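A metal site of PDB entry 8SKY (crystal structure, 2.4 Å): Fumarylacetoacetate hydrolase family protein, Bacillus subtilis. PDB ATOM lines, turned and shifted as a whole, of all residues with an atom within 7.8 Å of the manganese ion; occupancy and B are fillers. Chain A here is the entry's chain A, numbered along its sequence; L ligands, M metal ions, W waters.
The side-chain carboxylate (OD1) of Asp 182 lies within salt-bridge range of the side-chain amino group (NZ) of Lys 126. OG1 of Thr 184 is in hydrogen-bond range of O of Asp 182, 2.9 Å away. N of Glu 153 sits at hydrogen-bond distance from O of Val 180 (2.9 Å). OD1 of Asp 182 lies within salt-bridge range of NZ of Lys 199. N of Gly 268 lies within hydrogen-bond range of OE1 of Glu 153 (2.8 Å). The guanidinium group (NH2) of Arg 186 lies within salt-bridge range of the side-chain carboxylate (OE2) of Glu 151, at 3.0 Å. The backbone carbonyl oxygen of Lys 199 lies within hydrogen-bond range of the side-chain amino group of Lys 126. The side-chain carboxylate (OE2) of Glu 151 is in salt-bridge range of the side-chain amino group (NZ) of Lys 199 (3.3 Å).
NZ of Lys 199 touches the manganese ion, at 3.5 Å.
The manganese ion is bound by O1 of the ligand, 1.9 Å away. The side-chain carboxylate (OE2) of Glu 153 binds the manganese ion, 2.0 Å away. The side-chain carboxylate (OE1) of Glu 151 binds the manganese ion, at 2.0 Å. The side-chain carboxylate (OD2) of Asp 182 binds the manganese ion. Water W1 binds the manganese ion (2.3 Å). The manganese ion is bound by an oxygen (O4) of the ligand (2.4 Å).
Water W1 bridges O of Ile 100 (2.8 Å) and OE1 of Glu 153 (2.8 Å).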
ATOM      1  N   CYS A  99      -6.173  20.549  19.555  1.00  0.00           N
ATOM      2  CA  CYS A  99      -7.027  19.786  18.653  1.00  0.00           C
ATOM      3  C   CYS A  99      -6.185  18.907  17.741  1.00  0.00           C
ATOM      4  O   CYS A  99      -5.106  19.306  17.288  1.00  0.00           O
ATOM      5  CB  CYS A  99      -7.915  20.708  17.802  1.00  0.00           C
ATOM      6  SG  CYS A  99      -8.984  21.817  18.747  1.00  0.00           S
ATOM      7  N   ILE A 100      -6.708  17.719  17.457  1.00  0.00           N
ATOM      8  CA  ILE A 100      -6.074  16.745  16.576  1.00  0.00           C
ATOM      9  C   ILE A 100      -6.815  16.730  15.255  1.00  0.00           C
ATOM     10  O   ILE A 100      -8.048  16.639  15.231  1.00  0.00           O
ATOM     11  CB  ILE A 100      -6.063  15.343  17.214  1.00  0.00           C
ATOM     12  CG1 ILE A 100      -5.529  15.393  18.646  1.00  0.00           C
ATOM     13  CG2 ILE A 100      -5.234  14.381  16.365  1.00  0.00           C
ATOM     14  CD1 ILE A 100      -4.181  16.046  18.776  1.00  0.00           C
ATOM     15  N   GLY A 101      -6.077  16.817  14.152  1.00  0.00           N
ATOM     16  CA  GLY A 101      -6.655  16.743  12.823  1.00  0.00           C
ATOM     17  C   GLY A 101      -6.451  15.388  12.196  1.00  0.00           C
ATOM     18  O   GLY A 101      -5.419  14.742  12.391  1.00  0.00           O
ATOM     19  N   LYS A 102      -7.462  14.944  11.437  1.00  0.00           N
ATOM     20  CA  LYS A 102      -7.404  13.711  10.654  1.00  0.00           C
ATOM     21  C   LYS A 102      -6.996  12.520  11.506  1.00  0.00           C
ATOM     22  O   LYS A 102      -6.108  11.734  11.148  1.00  0.00           O
ATOM     23  CB  LYS A 102      -6.466  13.876   9.447  1.00  0.00           C
ATOM     24  CG  LYS A 102      -7.077  14.626   8.282  1.00  0.00           C
ATOM     25  CD  LYS A 102      -6.023  15.368   7.476  1.00  0.00           C
ATOM     26  CE  LYS A 102      -6.654  16.306   6.455  1.00  0.00           C
ATOM     27  NZ  LYS A 102      -5.670  16.800   5.456  1.00  0.00           N
ATOM     28  N   HIS A 107     -12.441  10.045   7.984  1.00  0.00           N
ATOM     29  CA  HIS A 107     -12.531  11.503   7.886  1.00  0.00           C
ATOM     30  C   HIS A 107     -11.380  12.081   7.072  1.00  0.00           C
ATOM     31  O   HIS A 107     -11.564  13.052   6.329  1.00  0.00           O
ATOM     32  CB  HIS A 107     -12.555  12.142   9.276  1.00  0.00           C
ATOM     33  CG  HIS A 107     -12.529  13.630   9.249  1.00  0.00           C
ATOM     34  ND1 HIS A 107     -13.525  14.384   8.673  1.00  0.00           N
ATOM     35  CD2 HIS A 107     -11.618  14.520   9.724  1.00  0.00           C
ATOM     36  CE1 HIS A 107     -13.237  15.668   8.784  1.00  0.00           C
ATOM     37  NE2 HIS A 107     -12.087  15.773   9.426  1.00  0.00           N
ATOM     38  N   PHE A 124      -3.344  21.385  16.158  1.00  0.00           N
ATOM     39  CA  PHE A 124      -3.589  22.818  16.053  1.00  0.00           C
ATOM     40  C   PHE A 124      -4.405  23.214  17.285  1.00  0.00           C
ATOM     41  O   PHE A 124      -4.650  22.395  18.174  1.00  0.00           O
ATOM     42  CB  PHE A 124      -4.292  23.132  14.735  1.00  0.00           C
ATOM     43  CG  PHE A 124      -5.610  22.434  14.567  1.00  0.00           C
ATOM     44  CD1 PHE A 124      -6.787  23.010  15.013  1.00  0.00           C
ATOM     45  CD2 PHE A 124      -5.664  21.170  13.997  1.00  0.00           C
ATOM     46  CE1 PHE A 124      -7.983  22.360  14.878  1.00  0.00           C
ATOM     47  CE2 PHE A 124      -6.867  20.513  13.860  1.00  0.00           C
ATOM     48  CZ  PHE A 124      -8.030  21.105  14.300  1.00  0.00           C
ATOM     49  N   LYS A 126      -7.675  25.889  19.130  1.00  0.00           N
ATOM     50  CA  LYS A 126      -8.812  26.793  19.092  1.00  0.00           C
ATOM     51  C   LYS A 126      -8.709  27.792  20.237  1.00  0.00           C
ATOM     52  O   LYS A 126      -8.531  27.383  21.381  1.00  0.00           O
ATOM     53  CB  LYS A 126     -10.138  26.039  19.212  1.00  0.00           C
ATOM     54  CG  LYS A 126     -10.469  25.116  18.066  1.00  0.00           C
ATOM     55  CD  LYS A 126     -11.779  24.409  18.335  1.00  0.00           C
ATOM     56  CE  LYS A 126     -12.959  25.314  18.036  1.00  0.00           C
ATOM     57  NZ  LYS A 126     -13.386  25.221  16.618  1.00  0.00           N
ATOM     58  N   TYR A 150     -19.608  21.332  11.136  1.00  0.00           N
ATOM     59  CA  TYR A 150     -19.699  20.727  12.453  1.00  0.00           C
ATOM     60  C   TYR A 150     -18.658  19.618  12.582  1.00  0.00           C
ATOM     61  O   TYR A 150     -18.291  18.982  11.593  1.00  0.00           O
ATOM     62  CB  TYR A 150     -21.092  20.151  12.699  1.00  0.00           C
ATOM     63  CG  TYR A 150     -21.503  19.175  11.628  1.00  0.00           C
ATOM     64  CD1 TYR A 150     -21.153  17.829  11.716  1.00  0.00           C
ATOM     65  CD2 TYR A 150     -22.201  19.590  10.502  1.00  0.00           C
ATOM     66  CE1 TYR A 150     -21.490  16.930  10.734  1.00  0.00           C
ATOM     67  CE2 TYR A 150     -22.560  18.696   9.517  1.00  0.00           C
ATOM     68  CZ  TYR A 150     -22.195  17.370   9.640  1.00  0.00           C
ATOM     69  OH  TYR A 150     -22.540  16.463   8.666  1.00  0.00           O
ATOM     70  N   GLU A 151     -18.203  19.378  13.814  1.00  0.00           N
ATOM     71  CA  GLU A 151     -17.245  18.310  14.085  1.00  0.00           C
ATOM     72  C   GLU A 151     -17.487  17.802  15.498  1.00  0.00           C
ATOM     73  O   GLU A 151     -17.009  18.406  16.468  1.00  0.00           O
ATOM     74  CB  GLU A 151     -15.803  18.799  13.921  1.00  0.00           C
ATOM     75  CG  GLU A 151     -15.365  19.073  12.490  1.00  0.00           C
ATOM     76  CD  GLU A 151     -13.865  19.193  12.366  1.00  0.00           C
ATOM     77  OE1 GLU A 151     -13.162  18.937  13.363  1.00  0.00           O
ATOM     78  OE2 GLU A 151     -13.383  19.567  11.276  1.00  0.00           O
ATOM     79  N   GLY A 152     -18.226  16.697  15.623  1.00  0.00           N
ATOM     80  CA  GLY A 152     -18.391  16.068  16.917  1.00  0.00           C
ATOM     81  C   GLY A 152     -17.114  15.374  17.341  1.00  0.00           C
ATOM     82  O   GLY A 152     -16.504  14.626  16.565  1.00  0.00           O
ATOM     83  N   GLU A 153     -16.675  15.630  18.581  1.00  0.00           N
ATOM     84  CA  GLU A 153     -15.409  15.094  19.057  1.00  0.00           C
ATOM     85  C   GLU A 153     -15.506  14.741  20.537  1.00  0.00           C
ATOM     86  O   GLU A 153     -16.190  15.421  21.305  1.00  0.00           O
ATOM     87  CB  GLU A 153     -14.252  16.072  18.836  1.00  0.00           C
ATOM     88  CG  GLU A 153     -14.096  16.588  17.420  1.00  0.00           C
ATOM     89  CD  GLU A 153     -12.717  17.130  17.139  1.00  0.00           C
ATOM     90  OE1 GLU A 153     -11.814  16.900  17.967  1.00  0.00           O
ATOM     91  OE2 GLU A 153     -12.538  17.785  16.094  1.00  0.00           O
ATOM     92  N   VAL A 180     -17.149  17.970  22.599  1.00  0.00           N
ATOM     93  CA  VAL A 180     -16.790  19.227  21.947  1.00  0.00           C
ATOM     94  C   VAL A 180     -17.313  19.207  20.520  1.00  0.00           C
ATOM     95  O   VAL A 180     -17.270  18.178  19.843  1.00  0.00           O
ATOM     96  CB  VAL A 180     -15.257  19.461  21.970  1.00  0.00           C
ATOM     97  CG1 VAL A 180     -14.829  20.420  20.879  1.00  0.00           C
ATOM     98  CG2 VAL A 180     -14.848  20.011  23.332  1.00  0.00           C
ATOM     99  N   ASN A 181     -17.842  20.346  20.070  1.00  0.00           N
ATOM    100  CA  ASN A 181     -18.168  20.579  18.665  1.00  0.00           C
ATOM    101  C   ASN A 181     -17.091  21.491  18.090  1.00  0.00           C
ATOM    102  O   ASN A 181     -17.031  22.678  18.441  1.00  0.00           O
ATOM    103  CB  ASN A 181     -19.549  21.197  18.512  1.00  0.00           C
ATOM    104  CG  ASN A 181     -20.098  21.059  17.111  1.00  0.00           C
ATOM    105  OD1 ASN A 181     -19.404  20.632  16.193  1.00  0.00           O
ATOM    106  ND2 ASN A 181     -21.360  21.432  16.928  1.00  0.00           N
ATOM    107  N   ASP A 182     -16.239  20.944  17.218  1.00  0.00           N
ATOM    108  CA  ASP A 182     -15.144  21.709  16.624  1.00  0.00           C
ATOM    109  C   ASP A 182     -15.655  22.395  15.358  1.00  0.00           C
ATOM    110  O   ASP A 182     -15.400  21.967  14.236  1.00  0.00           O
ATOM    111  CB  ASP A 182     -13.947  20.810  16.348  1.00  0.00           C
ATOM    112  CG  ASP A 182     -12.776  21.567  15.735  1.00  0.00           C
ATOM    113  OD1 ASP A 182     -12.743  22.806  15.842  1.00  0.00           O
ATOM    114  OD2 ASP A 182     -11.887  20.910  15.154  1.00  0.00           O
ATOM    115  N   ILE A 183     -16.397  23.480  15.561  1.00  0.00           N
ATOM    116  CA  ILE A 183     -17.037  24.175  14.458  1.00  0.00           C
ATOM    117  C   ILE A 183     -15.982  24.950  13.675  1.00  0.00           C
ATOM    118  O   ILE A 183     -15.204  25.731  14.251  1.00  0.00           O
ATOM    119  CB  ILE A 183     -18.158  25.076  14.970  1.00  0.00           C
ATOM    120  CG1 ILE A 183     -19.302  24.205  15.506  1.00  0.00           C
ATOM    121  CG2 ILE A 183     -18.661  26.000  13.877  1.00  0.00           C
ATOM    122  CD1 ILE A 183     -20.461  24.980  16.074  1.00  0.00           C
ATOM    123  N   THR A 184     -15.959  24.739  12.361  1.00  0.00           N
ATOM    124  CA  THR A 184     -14.864  25.175  11.496  1.00  0.00           C
ATOM    125  C   THR A 184     -15.403  25.879  10.258  1.00  0.00           C
ATOM    126  O   THR A 184     -16.410  25.459   9.684  1.00  0.00           O
ATOM    127  CB  THR A 184     -13.997  23.980  11.061  1.00  0.00           C
ATOM    128  OG1 THR A 184     -13.662  23.191  12.209  1.00  0.00           O
ATOM    129  CG2 THR A 184     -12.730  24.445  10.359  1.00  0.00           C
ATOM    130  N   ARG A 186     -14.608  26.203   6.663  1.00  0.00           N
ATOM    131  CA  ARG A 186     -13.777  25.461   5.730  1.00  0.00           C
ATOM    132  C   ARG A 186     -13.053  26.389   4.765  1.00  0.00           C
ATOM    133  O   ARG A 186     -11.897  26.128   4.381  1.00  0.00           O
ATOM    134  CB  ARG A 186     -14.611  24.433   4.972  1.00  0.00           C
ATOM    135  CG  ARG A 186     -15.296  23.405   5.864  1.00  0.00           C
ATOM    136  CD  ARG A 186     -14.325  22.311   6.318  1.00  0.00           C
ATOM    137  NE  ARG A 186     -14.990  21.297   7.133  1.00  0.00           N
ATOM    138  CZ  ARG A 186     -14.464  20.745   8.220  1.00  0.00           C
ATOM    139  NH1 ARG A 186     -13.249  21.113   8.640  1.00  0.00           N
ATOM    140  NH2 ARG A 186     -15.133  19.820   8.889  1.00  0.00           N
ATOM    141  N   GLN A 189     -10.200  28.050   6.500  1.00  0.00           N
ATOM    142  CA  GLN A 189      -9.147  27.055   6.731  1.00  0.00           C
ATOM    143  C   GLN A 189      -8.139  27.050   5.593  1.00  0.00           C
ATOM    144  O   GLN A 189      -6.925  27.004   5.826  1.00  0.00           O
ATOM    145  CB  GLN A 189      -9.780  25.684   6.913  1.00  0.00           C
ATOM    146  CG  GLN A 189      -8.925  24.682   7.650  1.00  0.00           C
ATOM    147  CD  GLN A 189      -9.734  23.509   8.175  1.00  0.00           C
ATOM    148  OE1 GLN A 189     -10.860  23.270   7.729  1.00  0.00           O
ATOM    149  NE2 GLN A 189      -9.174  22.770   9.119  1.00  0.00           N
ATOM    150  N   PHE A 195      -4.522  26.174  10.486  1.00  0.00           N
ATOM    151  CA  PHE A 195      -5.938  25.998  10.771  1.00  0.00           C
ATOM    152  C   PHE A 195      -6.483  27.050  11.735  1.00  0.00           C
ATOM    153  O   PHE A 195      -7.704  27.140  11.880  1.00  0.00           O
ATOM    154  CB  PHE A 195      -6.173  24.599  11.330  1.00  0.00           C
ATOM    155  CG  PHE A 195      -6.017  23.511  10.300  1.00  0.00           C
ATOM    156  CD1 PHE A 195      -5.939  23.825   8.946  1.00  0.00           C
ATOM    157  CD2 PHE A 195      -5.938  22.189  10.672  1.00  0.00           C
ATOM    158  CE1 PHE A 195      -5.795  22.837   7.994  1.00  0.00           C
ATOM    159  CE2 PHE A 195      -5.787  21.194   9.721  1.00  0.00           C
ATOM    160  CZ  PHE A 195      -5.713  21.521   8.387  1.00  0.00           C
ATOM    161  N   LYS A 199     -10.492  28.009  12.710  1.00  0.00           N
ATOM    162  CA  LYS A 199     -10.883  27.217  13.873  1.00  0.00           C
ATOM    163  C   LYS A 199     -11.214  28.068  15.088  1.00  0.00           C
ATOM    164  O   LYS A 199     -11.640  27.525  16.113  1.00  0.00           O
ATOM    165  CB  LYS A 199      -9.767  26.232  14.237  1.00  0.00           C
ATOM    166  CG  LYS A 199      -9.579  25.093  13.249  1.00  0.00           C
ATOM    167  CD  LYS A 199     -10.650  24.041  13.406  1.00  0.00           C
ATOM    168  CE  LYS A 199     -10.392  22.867  12.477  1.00  0.00           C
ATOM    169  NZ  LYS A 199     -11.361  21.768  12.688  1.00  0.00           N
ATOM    170  N   ALA A 266      -9.014  17.911  22.101  1.00  0.00           N
ATOM    171  CA  ALA A 266     -10.057  17.404  21.209  1.00  0.00           C
ATOM    172  C   ALA A 266      -9.417  16.415  20.256  1.00  0.00           C
ATOM    173  O   ALA A 266      -8.538  16.781  19.463  1.00  0.00           O
ATOM    174  CB  ALA A 266     -10.739  18.554  20.462  1.00  0.00           C
ATOM    175  N   THR A 267      -9.871  15.157  20.313  1.00  0.00           N
ATOM    176  CA  THR A 267      -9.149  14.041  19.729  1.00  0.00           C
ATOM    177  C   THR A 267      -9.514  13.771  18.265  1.00  0.00           C
ATOM    178  O   THR A 267      -9.033  12.778  17.702  1.00  0.00           O
ATOM    179  CB  THR A 267      -9.385  12.772  20.552  1.00  0.00           C
ATOM    180  OG1 THR A 267     -10.784  12.472  20.606  1.00  0.00           O
ATOM    181  CG2 THR A 267      -8.857  12.964  21.974  1.00  0.00           C
ATOM    182  N   GLY A 268     -10.323  14.610  17.654  1.00  0.00           N
ATOM    183  CA  GLY A 268     -10.550  14.454  16.223  1.00  0.00           C
ATOM    184  C   GLY A 268     -11.939  13.903  15.922  1.00  0.00           C
ATOM    185  O   GLY A 268     -12.450  13.022  16.621  1.00  0.00           O
ATOM    186  N   THR A 269     -12.544  14.427  14.841  1.00  0.00           N
ATOM    187  CA  THR A 269     -13.920  14.099  14.510  1.00  0.00           C
ATOM    188  C   THR A 269     -13.992  12.926  13.539  1.00  0.00           C
ATOM    189  O   THR A 269     -13.089  12.728  12.713  1.00  0.00           O
ATOM    190  CB  THR A 269     -14.632  15.321  13.916  1.00  0.00           C
ATOM    191  OG1 THR A 269     -16.058  15.144  14.007  1.00  0.00           O
ATOM    192  CG2 THR A 269     -14.231  15.551  12.465  1.00  0.00           C
ATOM    193  N   PRO A 270     -15.039  12.092  13.647  1.00  0.00           N
ATOM    194  CA  PRO A 270     -15.203  10.998  12.687  1.00  0.00           C
ATOM    195  C   PRO A 270     -15.635  11.491  11.316  1.00  0.00           C
ATOM    196  O   PRO A 270     -15.815  12.701  11.112  1.00  0.00           O
ATOM    197  CB  PRO A 270     -16.287  10.116  13.333  1.00  0.00           C
ATOM    198  CG  PRO A 270     -16.434  10.603  14.742  1.00  0.00           C
ATOM    199  CD  PRO A 270     -16.033  12.046  14.722  1.00  0.00           C
ATOM    200  N   VAL A 273     -18.601  14.724   8.205  1.00  0.00           N
ATOM    201  CA  VAL A 273     -18.680  16.167   8.311  1.00  0.00           C
ATOM    202  C   VAL A 273     -19.370  16.747   7.078  1.00  0.00           C
ATOM    203  O   VAL A 273     -19.481  16.095   6.031  1.00  0.00           O
ATOM    204  CB  VAL A 273     -17.292  16.797   8.506  1.00  0.00           C
ATOM    205  CG1 VAL A 273     -16.604  16.198   9.716  1.00  0.00           C
ATOM    206  CG2 VAL A 273     -16.450  16.639   7.257  1.00  0.00           C
HETATM  207  C1  LIG L   1      -9.884  18.372  12.627  1.00  0.00           C
HETATM  208  C2  LIG L   1     -10.289  16.937  12.932  1.00  0.00           C
HETATM  209  O1  LIG L   1     -10.322  19.322  13.336  1.00  0.00           O
HETATM  210  O2  LIG L   1      -9.755  15.981  12.300  1.00  0.00           O
HETATM  211  O3  LIG L   1      -9.113  18.615  11.664  1.00  0.00           O
HETATM  212  O4  LIG L   1     -11.160  16.693  13.808  1.00  0.00           O
HETATM  213 MN    MN M   1     -11.633  18.872  14.682  1.00  0.00          MN
HETATM  214  O   HOH W   1     -10.072  18.309  16.240  1.00  0.00           O
